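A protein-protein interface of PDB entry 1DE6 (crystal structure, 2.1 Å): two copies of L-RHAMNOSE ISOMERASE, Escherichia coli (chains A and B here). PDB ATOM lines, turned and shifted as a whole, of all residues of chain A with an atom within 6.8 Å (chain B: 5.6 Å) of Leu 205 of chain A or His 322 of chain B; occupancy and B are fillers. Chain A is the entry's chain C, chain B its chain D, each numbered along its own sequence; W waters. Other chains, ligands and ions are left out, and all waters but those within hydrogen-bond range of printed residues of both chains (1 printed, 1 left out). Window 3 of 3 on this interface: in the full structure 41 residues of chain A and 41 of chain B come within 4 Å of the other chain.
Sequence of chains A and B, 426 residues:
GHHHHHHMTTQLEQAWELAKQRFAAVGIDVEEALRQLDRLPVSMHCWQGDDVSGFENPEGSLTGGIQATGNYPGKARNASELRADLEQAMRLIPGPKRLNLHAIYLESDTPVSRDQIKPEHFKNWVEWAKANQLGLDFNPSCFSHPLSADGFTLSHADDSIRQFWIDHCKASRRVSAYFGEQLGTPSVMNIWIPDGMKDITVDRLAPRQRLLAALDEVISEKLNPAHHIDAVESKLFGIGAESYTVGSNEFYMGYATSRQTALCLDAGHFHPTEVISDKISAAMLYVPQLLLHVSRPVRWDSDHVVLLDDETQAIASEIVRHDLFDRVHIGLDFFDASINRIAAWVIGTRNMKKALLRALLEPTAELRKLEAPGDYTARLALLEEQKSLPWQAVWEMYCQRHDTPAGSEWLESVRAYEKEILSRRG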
ATOM      1  N   THR A 201     -13.874  17.072  14.952  1.00  0.00           N
ATOM      2  CA  THR A 201     -13.109  16.063  14.253  1.00  0.00           C
ATOM      3  C   THR A 201     -13.754  14.689  14.225  1.00  0.00           C
ATOM      4  O   THR A 201     -14.303  14.208  15.240  1.00  0.00           O
ATOM      5  CB  THR A 201     -11.810  15.958  15.012  1.00  0.00           C
ATOM      6  OG1 THR A 201     -11.188  17.259  14.964  1.00  0.00           O
ATOM      7  CG2 THR A 201     -10.932  14.855  14.466  1.00  0.00           C
ATOM      8  N   VAL A 202     -13.697  14.061  13.046  1.00  0.00           N
ATOM      9  CA  VAL A 202     -14.228  12.690  12.852  1.00  0.00           C
ATOM     10  C   VAL A 202     -13.212  11.637  13.333  1.00  0.00           C
ATOM     11  O   VAL A 202     -13.529  10.714  14.131  1.00  0.00           O
ATOM     12  CB  VAL A 202     -14.471  12.455  11.366  1.00  0.00           C
ATOM     13  CG1 VAL A 202     -14.923  11.023  11.188  1.00  0.00           C
ATOM     14  CG2 VAL A 202     -15.524  13.434  10.883  1.00  0.00           C
ATOM     15  N   ASP A 203     -11.946  11.805  12.917  1.00  0.00           N
ATOM     16  CA  ASP A 203     -10.988  10.804  13.340  1.00  0.00           C
ATOM     17  C   ASP A 203      -9.793  11.296  14.109  1.00  0.00           C
ATOM     18  O   ASP A 203      -8.758  11.707  13.519  1.00  0.00           O
ATOM     19  CB  ASP A 203     -10.500   9.969  12.128  1.00  0.00           C
ATOM     20  CG  ASP A 203      -9.582   8.762  12.497  1.00  0.00           C
ATOM     21  OD1 ASP A 203      -9.179   8.427  13.640  1.00  0.00           O
ATOM     22  OD2 ASP A 203      -9.209   8.091  11.434  1.00  0.00           O
ATOM     23  N   ARG A 204      -9.860  11.145  15.444  1.00  0.00           N
ATOM     24  CA  ARG A 204      -8.725  11.575  16.227  1.00  0.00           C
ATOM     25  C   ARG A 204      -7.735  10.464  16.329  1.00  0.00           C
ATOM     26  O   ARG A 204      -6.655  10.719  16.823  1.00  0.00           O
ATOM     27  CB  ARG A 204      -9.140  11.940  17.664  1.00  0.00           C
ATOM     28  CG  ARG A 204     -10.058  13.155  17.615  1.00  0.00           C
ATOM     29  CD  ARG A 204     -11.152  13.302  18.638  1.00  0.00           C
ATOM     30  NE  ARG A 204     -10.779  14.291  19.563  1.00  0.00           N
ATOM     31  CZ  ARG A 204     -11.114  15.567  19.798  1.00  0.00           C
ATOM     32  NH1 ARG A 204     -12.068  16.357  19.209  1.00  0.00           N
ATOM     33  NH2 ARG A 204     -10.324  16.017  20.801  1.00  0.00           N
ATOM     34  N   LEU A 205      -8.084   9.227  15.926  1.00  0.00           N
ATOM     35  CA  LEU A 205      -7.150   8.131  16.127  1.00  0.00           C
ATOM     36  C   LEU A 205      -5.966   8.029  15.147  1.00  0.00           C
ATOM     37  O   LEU A 205      -4.778   7.854  15.526  1.00  0.00           O
ATOM     38  CB  LEU A 205      -7.994   6.856  16.154  1.00  0.00           C
ATOM     39  CG  LEU A 205      -7.145   5.596  16.242  1.00  0.00           C
ATOM     40  CD1 LEU A 205      -6.400   5.331  17.601  1.00  0.00           C
ATOM     41  CD2 LEU A 205      -8.040   4.428  15.942  1.00  0.00           C
ATOM     42  N   ALA A 206      -6.282   8.088  13.863  1.00  0.00           N
ATOM     43  CA  ALA A 206      -5.259   7.928  12.814  1.00  0.00           C
ATOM     44  C   ALA A 206      -4.036   8.828  12.909  1.00  0.00           C
ATOM     45  O   ALA A 206      -2.824   8.413  12.849  1.00  0.00           O
ATOM     46  CB  ALA A 206      -5.875   7.909  11.443  1.00  0.00           C
ATOM     47  N   PRO A 207      -4.338  10.099  13.122  1.00  0.00           N
ATOM     48  CA  PRO A 207      -3.238  11.014  13.294  1.00  0.00           C
ATOM     49  C   PRO A 207      -2.391  10.620  14.488  1.00  0.00           C
ATOM     50  O   PRO A 207      -1.142  10.775  14.456  1.00  0.00           O
ATOM     51  CB  PRO A 207      -3.869  12.375  13.492  1.00  0.00           C
ATOM     52  CG  PRO A 207      -5.292  12.251  12.922  1.00  0.00           C
ATOM     53  CD  PRO A 207      -5.673  10.778  12.999  1.00  0.00           C
ATOM     54  N   ARG A 208      -3.028  10.089  15.569  1.00  0.00           N
ATOM     55  CA  ARG A 208      -2.194   9.679  16.727  1.00  0.00           C
ATOM     56  C   ARG A 208      -1.357   8.463  16.408  1.00  0.00           C
ATOM     57  O   ARG A 208      -0.184   8.312  16.817  1.00  0.00           O
ATOM     58  CB  ARG A 208      -2.993   9.548  18.041  1.00  0.00           C
ATOM     59  CG  ARG A 208      -3.506  10.950  18.464  1.00  0.00           C
ATOM     60  CD  ARG A 208      -4.522  10.922  19.581  1.00  0.00           C
ATOM     61  NE  ARG A 208      -4.692  12.269  20.206  1.00  0.00           N
ATOM     62  CZ  ARG A 208      -5.815  12.644  20.863  1.00  0.00           C
ATOM     63  NH1 ARG A 208      -6.889  11.842  21.032  1.00  0.00           N
ATOM     64  NH2 ARG A 208      -5.875  13.880  21.323  1.00  0.00           N
ATOM     65  N   GLN A 209      -1.987   7.601  15.604  1.00  0.00           N
ATOM     66  CA  GLN A 209      -1.288   6.406  15.157  1.00  0.00           C
ATOM     67  C   GLN A 209      -0.052   6.741  14.358  1.00  0.00           C
ATOM     68  O   GLN A 209       1.055   6.218  14.592  1.00  0.00           O
ATOM     69  CB  GLN A 209      -2.197   5.577  14.292  1.00  0.00           C
ATOM     70  CG  GLN A 209      -3.255   4.895  15.180  1.00  0.00           C
ATOM     71  CD  GLN A 209      -4.257   4.178  14.279  1.00  0.00           C
ATOM     72  OE1 GLN A 209      -4.494   4.638  13.136  1.00  0.00           O
ATOM     73  NE2 GLN A 209      -4.809   3.048  14.756  1.00  0.00           N
ATOM     74  N   ARG A 210      -0.287   7.656  13.415  1.00  0.00           N
ATOM     75  CA  ARG A 210       0.824   8.139  12.600  1.00  0.00           C
ATOM     76  C   ARG A 210       1.861   8.838  13.461  1.00  0.00           C
ATOM     77  O   ARG A 210       3.059   8.679  13.265  1.00  0.00           O
ATOM     78  CB  ARG A 210       0.365   9.118  11.519  1.00  0.00           C
ATOM     79  CG  ARG A 210      -0.404   8.362  10.481  1.00  0.00           C
ATOM     80  CD  ARG A 210      -0.769   9.169   9.227  1.00  0.00           C
ATOM     81  NE  ARG A 210      -1.498  10.413   9.430  1.00  0.00           N
ATOM     82  CZ  ARG A 210      -2.807  10.523   9.376  1.00  0.00           C
ATOM     83  NH1 ARG A 210      -3.368  11.703   9.516  1.00  0.00           N
ATOM     84  NH2 ARG A 210      -3.555   9.436   9.241  1.00  0.00           N
ATOM     85  N   LEU A 211       1.419   9.664  14.415  1.00  0.00           N
ATOM     86  CA  LEU A 211       2.379  10.348  15.213  1.00  0.00           C
ATOM     87  C   LEU A 211       3.198   9.311  15.958  1.00  0.00           C
ATOM     88  O   LEU A 211       4.442   9.363  16.057  1.00  0.00           O
ATOM     89  CB  LEU A 211       1.661  11.319  16.159  1.00  0.00           C
ATOM     90  CG  LEU A 211       2.626  12.059  17.069  1.00  0.00           C
ATOM     91  CD1 LEU A 211       3.555  12.972  16.211  1.00  0.00           C
ATOM     92  CD2 LEU A 211       1.768  12.935  17.949  1.00  0.00           C
ATOM     93  N   TYR A 244      -8.975  19.924  18.654  1.00  0.00           N
ATOM     94  CA  TYR A 244      -8.241  18.656  18.861  1.00  0.00           C
ATOM     95  C   TYR A 244      -6.790  18.839  18.569  1.00  0.00           C
ATOM     96  O   TYR A 244      -6.457  19.496  17.559  1.00  0.00           O
ATOM     97  CB  TYR A 244      -8.787  17.702  17.731  1.00  0.00           C
ATOM     98  CG  TYR A 244      -7.907  16.508  17.350  1.00  0.00           C
ATOM     99  CD1 TYR A 244      -7.539  15.528  18.270  1.00  0.00           C
ATOM    100  CD2 TYR A 244      -7.483  16.358  16.026  1.00  0.00           C
ATOM    101  CE1 TYR A 244      -6.755  14.438  17.886  1.00  0.00           C
ATOM    102  CE2 TYR A 244      -6.728  15.258  15.610  1.00  0.00           C
ATOM    103  CZ  TYR A 244      -6.375  14.282  16.545  1.00  0.00           C
ATOM    104  OH  TYR A 244      -5.604  13.213  16.109  1.00  0.00           O
ATOM    105  N   VAL A 246      -3.394  16.355  18.205  1.00  0.00           N
ATOM    106  CA  VAL A 246      -2.936  14.974  18.077  1.00  0.00           C
ATOM    107  C   VAL A 246      -2.115  14.600  19.293  1.00  0.00           C
ATOM    108  O   VAL A 246      -2.412  13.611  19.943  1.00  0.00           O
ATOM    109  CB  VAL A 246      -2.097  14.858  16.782  1.00  0.00           C
ATOM    110  CG1 VAL A 246      -1.605  13.461  16.470  1.00  0.00           C
ATOM    111  CG2 VAL A 246      -2.890  15.398  15.557  1.00  0.00           C
ATOM    112  N   ILE B 280      -9.990   8.883  24.703  1.00  0.00           N
ATOM    113  CA  ILE B 280     -10.119   7.514  24.247  1.00  0.00           C
ATOM    114  C   ILE B 280      -9.127   7.120  23.184  1.00  0.00           C
ATOM    115  O   ILE B 280      -8.354   6.205  23.381  1.00  0.00           O
ATOM    116  CB  ILE B 280     -11.560   7.263  23.838  1.00  0.00           C
ATOM    117  CG1 ILE B 280     -12.537   7.346  25.031  1.00  0.00           C
ATOM    118  CG2 ILE B 280     -11.658   5.962  23.014  1.00  0.00           C
ATOM    119  CD1 ILE B 280     -13.994   7.556  24.583  1.00  0.00           C
ATOM    120  N   SER B 281      -9.095   7.872  22.092  1.00  0.00           N
ATOM    121  CA  SER B 281      -8.124   7.504  21.078  1.00  0.00           C
ATOM    122  C   SER B 281      -6.687   7.656  21.529  1.00  0.00           C
ATOM    123  O   SER B 281      -5.818   6.955  21.070  1.00  0.00           O
ATOM    124  CB  SER B 281      -8.358   8.185  19.739  1.00  0.00           C
ATOM    125  OG  SER B 281      -8.238   9.578  19.980  1.00  0.00           O
ATOM    126  N   MET B 284      -5.893   4.407  24.010  1.00  0.00           N
ATOM    127  CA  MET B 284      -5.900   3.047  23.432  1.00  0.00           C
ATOM    128  C   MET B 284      -4.602   2.649  22.682  1.00  0.00           C
ATOM    129  O   MET B 284      -4.376   1.458  22.372  1.00  0.00           O
ATOM    130  CB  MET B 284      -7.111   2.818  22.513  1.00  0.00           C
ATOM    131  CG  MET B 284      -7.041   3.717  21.292  1.00  0.00           C
ATOM    132  SD  MET B 284      -8.595   3.720  20.271  1.00  0.00           S
ATOM    133  CE  MET B 284      -8.370   2.186  19.303  1.00  0.00           C
ATOM    134  N   LEU B 285      -3.722   3.632  22.353  1.00  0.00           N
ATOM    135  CA  LEU B 285      -2.443   3.372  21.699  1.00  0.00           C
ATOM    136  C   LEU B 285      -1.498   2.833  22.721  1.00  0.00           C
ATOM    137  O   LEU B 285      -0.400   2.366  22.444  1.00  0.00           O
ATOM    138  CB  LEU B 285      -1.801   4.649  21.067  1.00  0.00           C
ATOM    139  CG  LEU B 285      -2.647   5.188  19.945  1.00  0.00           C
ATOM    140  CD1 LEU B 285      -2.015   6.424  19.340  1.00  0.00           C
ATOM    141  CD2 LEU B 285      -2.700   4.143  18.845  1.00  0.00           C
ATOM    142  N   SER B 317     -19.376   8.382  20.111  1.00  0.00           N
ATOM    143  CA  SER B 317     -18.835   8.455  18.801  1.00  0.00           C
ATOM    144  C   SER B 317     -17.506   7.845  18.742  1.00  0.00           C
ATOM    145  O   SER B 317     -17.196   7.063  17.902  1.00  0.00           O
ATOM    146  CB  SER B 317     -18.778   9.877  18.238  1.00  0.00           C
ATOM    147  OG  SER B 317     -20.115  10.355  18.156  1.00  0.00           O
ATOM    148  N   GLU B 318     -16.710   8.217  19.670  1.00  0.00           N
ATOM    149  CA  GLU B 318     -15.326   7.739  19.715  1.00  0.00           C
ATOM    150  C   GLU B 318     -15.233   6.249  19.769  1.00  0.00           C
ATOM    151  O   GLU B 318     -14.413   5.625  19.079  1.00  0.00           O
ATOM    152  CB  GLU B 318     -14.466   8.407  20.842  1.00  0.00           C
ATOM    153  CG  GLU B 318     -14.433   9.954  20.691  1.00  0.00           C
ATOM    154  CD  GLU B 318     -13.705  10.277  19.389  1.00  0.00           C
ATOM    155  OE1 GLU B 318     -12.533   9.964  19.262  1.00  0.00           O
ATOM    156  OE2 GLU B 318     -14.429  10.798  18.436  1.00  0.00           O
ATOM    157  N   ILE B 319     -16.042   5.668  20.661  1.00  0.00           N
ATOM    158  CA  ILE B 319     -16.027   4.226  20.823  1.00  0.00           C
ATOM    159  C   ILE B 319     -16.418   3.545  19.503  1.00  0.00           C
ATOM    160  O   ILE B 319     -15.791   2.618  19.060  1.00  0.00           O
ATOM    161  CB  ILE B 319     -17.142   3.866  21.769  1.00  0.00           C
ATOM    162  CG1 ILE B 319     -16.892   4.454  23.137  1.00  0.00           C
ATOM    163  CG2 ILE B 319     -17.294   2.336  21.856  1.00  0.00           C
ATOM    164  CD1 ILE B 319     -18.109   4.288  24.089  1.00  0.00           C
ATOM    165  N   VAL B 320     -17.498   4.046  18.942  1.00  0.00           N
ATOM    166  CA  VAL B 320     -17.945   3.484  17.742  1.00  0.00           C
ATOM    167  C   VAL B 320     -17.008   3.780  16.526  1.00  0.00           C
ATOM    168  O   VAL B 320     -16.690   2.877  15.786  1.00  0.00           O
ATOM    169  CB  VAL B 320     -19.355   3.960  17.518  1.00  0.00           C
ATOM    170  CG1 VAL B 320     -19.837   3.761  16.069  1.00  0.00           C
ATOM    171  CG2 VAL B 320     -20.213   3.191  18.489  1.00  0.00           C
ATOM    172  N   ARG B 321     -16.588   5.030  16.268  1.00  0.00           N
ATOM    173  CA  ARG B 321     -15.733   5.347  15.155  1.00  0.00           C
ATOM    174  C   ARG B 321     -14.536   4.474  15.129  1.00  0.00           C
ATOM    175  O   ARG B 321     -14.060   4.101  14.037  1.00  0.00           O
ATOM    176  CB  ARG B 321     -15.235   6.765  15.233  1.00  0.00           C
ATOM    177  CG  ARG B 321     -16.377   7.698  14.891  1.00  0.00           C
ATOM    178  CD  ARG B 321     -16.056   9.155  15.261  1.00  0.00           C
ATOM    179  NE  ARG B 321     -17.076  10.106  14.785  1.00  0.00           N
ATOM    180  CZ  ARG B 321     -17.165  11.352  15.262  1.00  0.00           C
ATOM    181  NH1 ARG B 321     -16.289  11.801  16.175  1.00  0.00           N
ATOM    182  NH2 ARG B 321     -18.115  12.170  14.793  1.00  0.00           N
ATOM    183  N   HIS B 322     -14.052   4.176  16.323  1.00  0.00           N
ATOM    184  CA  HIS B 322     -12.845   3.376  16.425  1.00  0.00           C
ATOM    185  C   HIS B 322     -13.038   1.878  16.527  1.00  0.00           C
ATOM    186  O   HIS B 322     -12.124   1.108  16.707  1.00  0.00           O
ATOM    187  CB  HIS B 322     -11.818   3.992  17.410  1.00  0.00           C
ATOM    188  CG  HIS B 322     -11.648   5.489  17.056  1.00  0.00           C
ATOM    189  ND1 HIS B 322     -11.455   5.943  15.709  1.00  0.00           N
ATOM    190  CD2 HIS B 322     -11.688   6.605  17.857  1.00  0.00           C
ATOM    191  CE1 HIS B 322     -11.393   7.275  15.731  1.00  0.00           C
ATOM    192  NE2 HIS B 322     -11.557   7.704  16.992  1.00  0.00           N
ATOM    193  N   ASP B 323     -14.263   1.468  16.417  1.00  0.00           N
ATOM    194  CA  ASP B 323     -14.611   0.075  16.456  1.00  0.00           C
ATOM    195  C   ASP B 323     -14.094  -0.631  17.713  1.00  0.00           C
ATOM    196  O   ASP B 323     -13.515  -1.739  17.759  1.00  0.00           O
ATOM    197  CB  ASP B 323     -14.084  -0.443  15.136  1.00  0.00           C
ATOM    198  CG  ASP B 323     -15.096  -1.399  14.660  1.00  0.00           C
ATOM    199  OD1 ASP B 323     -16.159  -1.045  14.176  1.00  0.00           O
ATOM    200  OD2 ASP B 323     -14.738  -2.627  14.957  1.00  0.00           O
ATOM    201  N   LEU B 324     -14.316   0.092  18.780  1.00  0.00           N
ATOM    202  CA  LEU B 324     -13.808  -0.323  20.030  1.00  0.00           C
ATOM    203  C   LEU B 324     -14.633  -1.391  20.711  1.00  0.00           C
ATOM    204  O   LEU B 324     -14.550  -1.592  21.907  1.00  0.00           O
ATOM    205  CB  LEU B 324     -13.565   0.998  20.848  1.00  0.00           C
ATOM    206  CG  LEU B 324     -12.350   1.712  20.276  1.00  0.00           C
ATOM    207  CD1 LEU B 324     -12.122   2.982  21.049  1.00  0.00           C
ATOM    208  CD2 LEU B 324     -11.147   0.817  20.481  1.00  0.00           C
ATOM    209  N   ARG B 368     -15.179  10.436   7.321  1.00  0.00           N
ATOM    210  CA  ARG B 368     -13.756  10.267   7.459  1.00  0.00           C
ATOM    211  C   ARG B 368     -12.986  10.653   6.185  1.00  0.00           C
ATOM    212  O   ARG B 368     -11.848  11.223   6.132  1.00  0.00           O
ATOM    213  CB  ARG B 368     -13.587   8.817   7.653  1.00  0.00           C
ATOM    214  CG  ARG B 368     -12.389   8.538   8.493  1.00  0.00           C
ATOM    215  CD  ARG B 368     -11.986   7.090   8.357  1.00  0.00           C
ATOM    216  NE  ARG B 368     -12.470   6.244   9.445  1.00  0.00           N
ATOM    217  CZ  ARG B 368     -12.694   6.560  10.731  1.00  0.00           C
ATOM    218  NH1 ARG B 368     -12.562   7.791  11.241  1.00  0.00           N
ATOM    219  NH2 ARG B 368     -13.097   5.583  11.541  1.00  0.00           N
HETATM  220  O   HOH W   1     -12.204  10.314  16.187  1.00  0.00           O
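Water W1 lies within hydrogen-bond range of the backbone carbonyl oxygen of Val 202 of chain A (2.5 Å), the backbone NH of Arg 204 of chain A (2.6 Å), a ring nitrogen (NE2) of His 322 of chain B (2.8 Å) and the side-chain carboxylate of Glu 318 of chain B (3.1 Å).
Printed residues of chain B that touch a printed residue of chain A: Ser 281, Met 284, Leu 285, Glu 318, Arg 321, His 322 and Arg 368. Hydrophobic or aromatic side chains of chain B that line the printed part of chain A: Met 284, Leu 285 and His 322. Printed residues of chain A that touch a printed residue of chain B: Thr 201, Val 202, Asp 203, Arg 204, Leu 205, Arg 208 and Gln 209. Hydrophobic or aromatic side chains of chain A that line the printed part of chain B: Val 202 and Leu 205. Among the printed residues, Asp or Glu carboxylates within 4 Å of a Lys or Arg side-chain nitrogen of the other chain: Asp 203 of chain A with Arg 368 of chain B.
No position is printed for both chains. Of the 13 pairs that touch across the chains among the printed residues, none has its exchanged pair printed and touching as well.
Of the printed residues of chain A, His 322 of chain B touches Asp 203 and Leu 205. Of the printed residues of chain A, Leu 285 of chain B touches Arg 208 and Gln 209. Of the printed residues of chain B, Thr 201 of chain A touches Arg 321 (3.3 Å). The nearest residue of chain B that does not touch Leu 205 of chain A is Leu 285 of chain B (4.1 Å). The nearest residue of chain A that does not touch His 322 of chain B is Arg 204 of chain A (4.1 Å).
N of Ala 206 of chain A sits at hydrogen-bond distance from OD1 of Asp 203 of chain A (2.9 Å). The guanidinium group (NH2) of Arg 368 of chain B lies within hydrogen-bond range of the backbone carbonyl oxygen (O) of Arg 321 of chain B (3.1 Å). The side-chain carboxylate (OE2) of Glu 318 of chain B is in salt-bridge range of the guanidinium group (NH1) of Arg 321 of chain B (3.1 Å). The side-chain carboxylate (OE1) of Glu 318 of chain B lies within hydrogen-bond range of a ring nitrogen (NE2) of His 322 of chain B, 3.3 Å away. The guanidinium group (NE) of Arg 208 of chain A sits at hydrogen-bond distance from the backbone carbonyl oxygen (O) of Val 246 of chain A (2.7 Å). The side-chain hydroxyl (OH) of Tyr 244 of chain A is in hydrogen-bond range of the backbone carbonyl oxygen (O) of Arg 204 of chain A (2.8 Å).
The side-chain carboxylate of Asp 203 of chain A lies within salt-bridge range of the guanidinium group of Arg 368 of chain B (3.4 Å). The side-chain hydroxyl of Ser 281 of chain B lies within hydrogen-bond range of the guanidinium group of Arg 208 of chain A, at 2.8 Å. O of Thr 201 of chain A sits at hydrogen-bond distance from NH1 of Arg 321 of chain B, at 3.3 Å.
Among the printed residues, pairs that only touch across the chains: Val 202 of chain A with Arg 321 of chain B, Val 202 of chain A with Arg 368 of chain B, Asp 203 of chain A with His 322 of chain B, Arg 204 of chain A with Ser 281 of chain B, Arg 204 of chain A with Glu 318 of chain B, Leu 205 of chain A with Ser 281 of chain B, Leu 205 of chain A with Met 284 of chain B, Leu 205 of chain A with His 322 of chain B, Arg 208 of chain A with Leu 285 of chain B and Gln 209 of chain A with Leu 285 of chain B.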
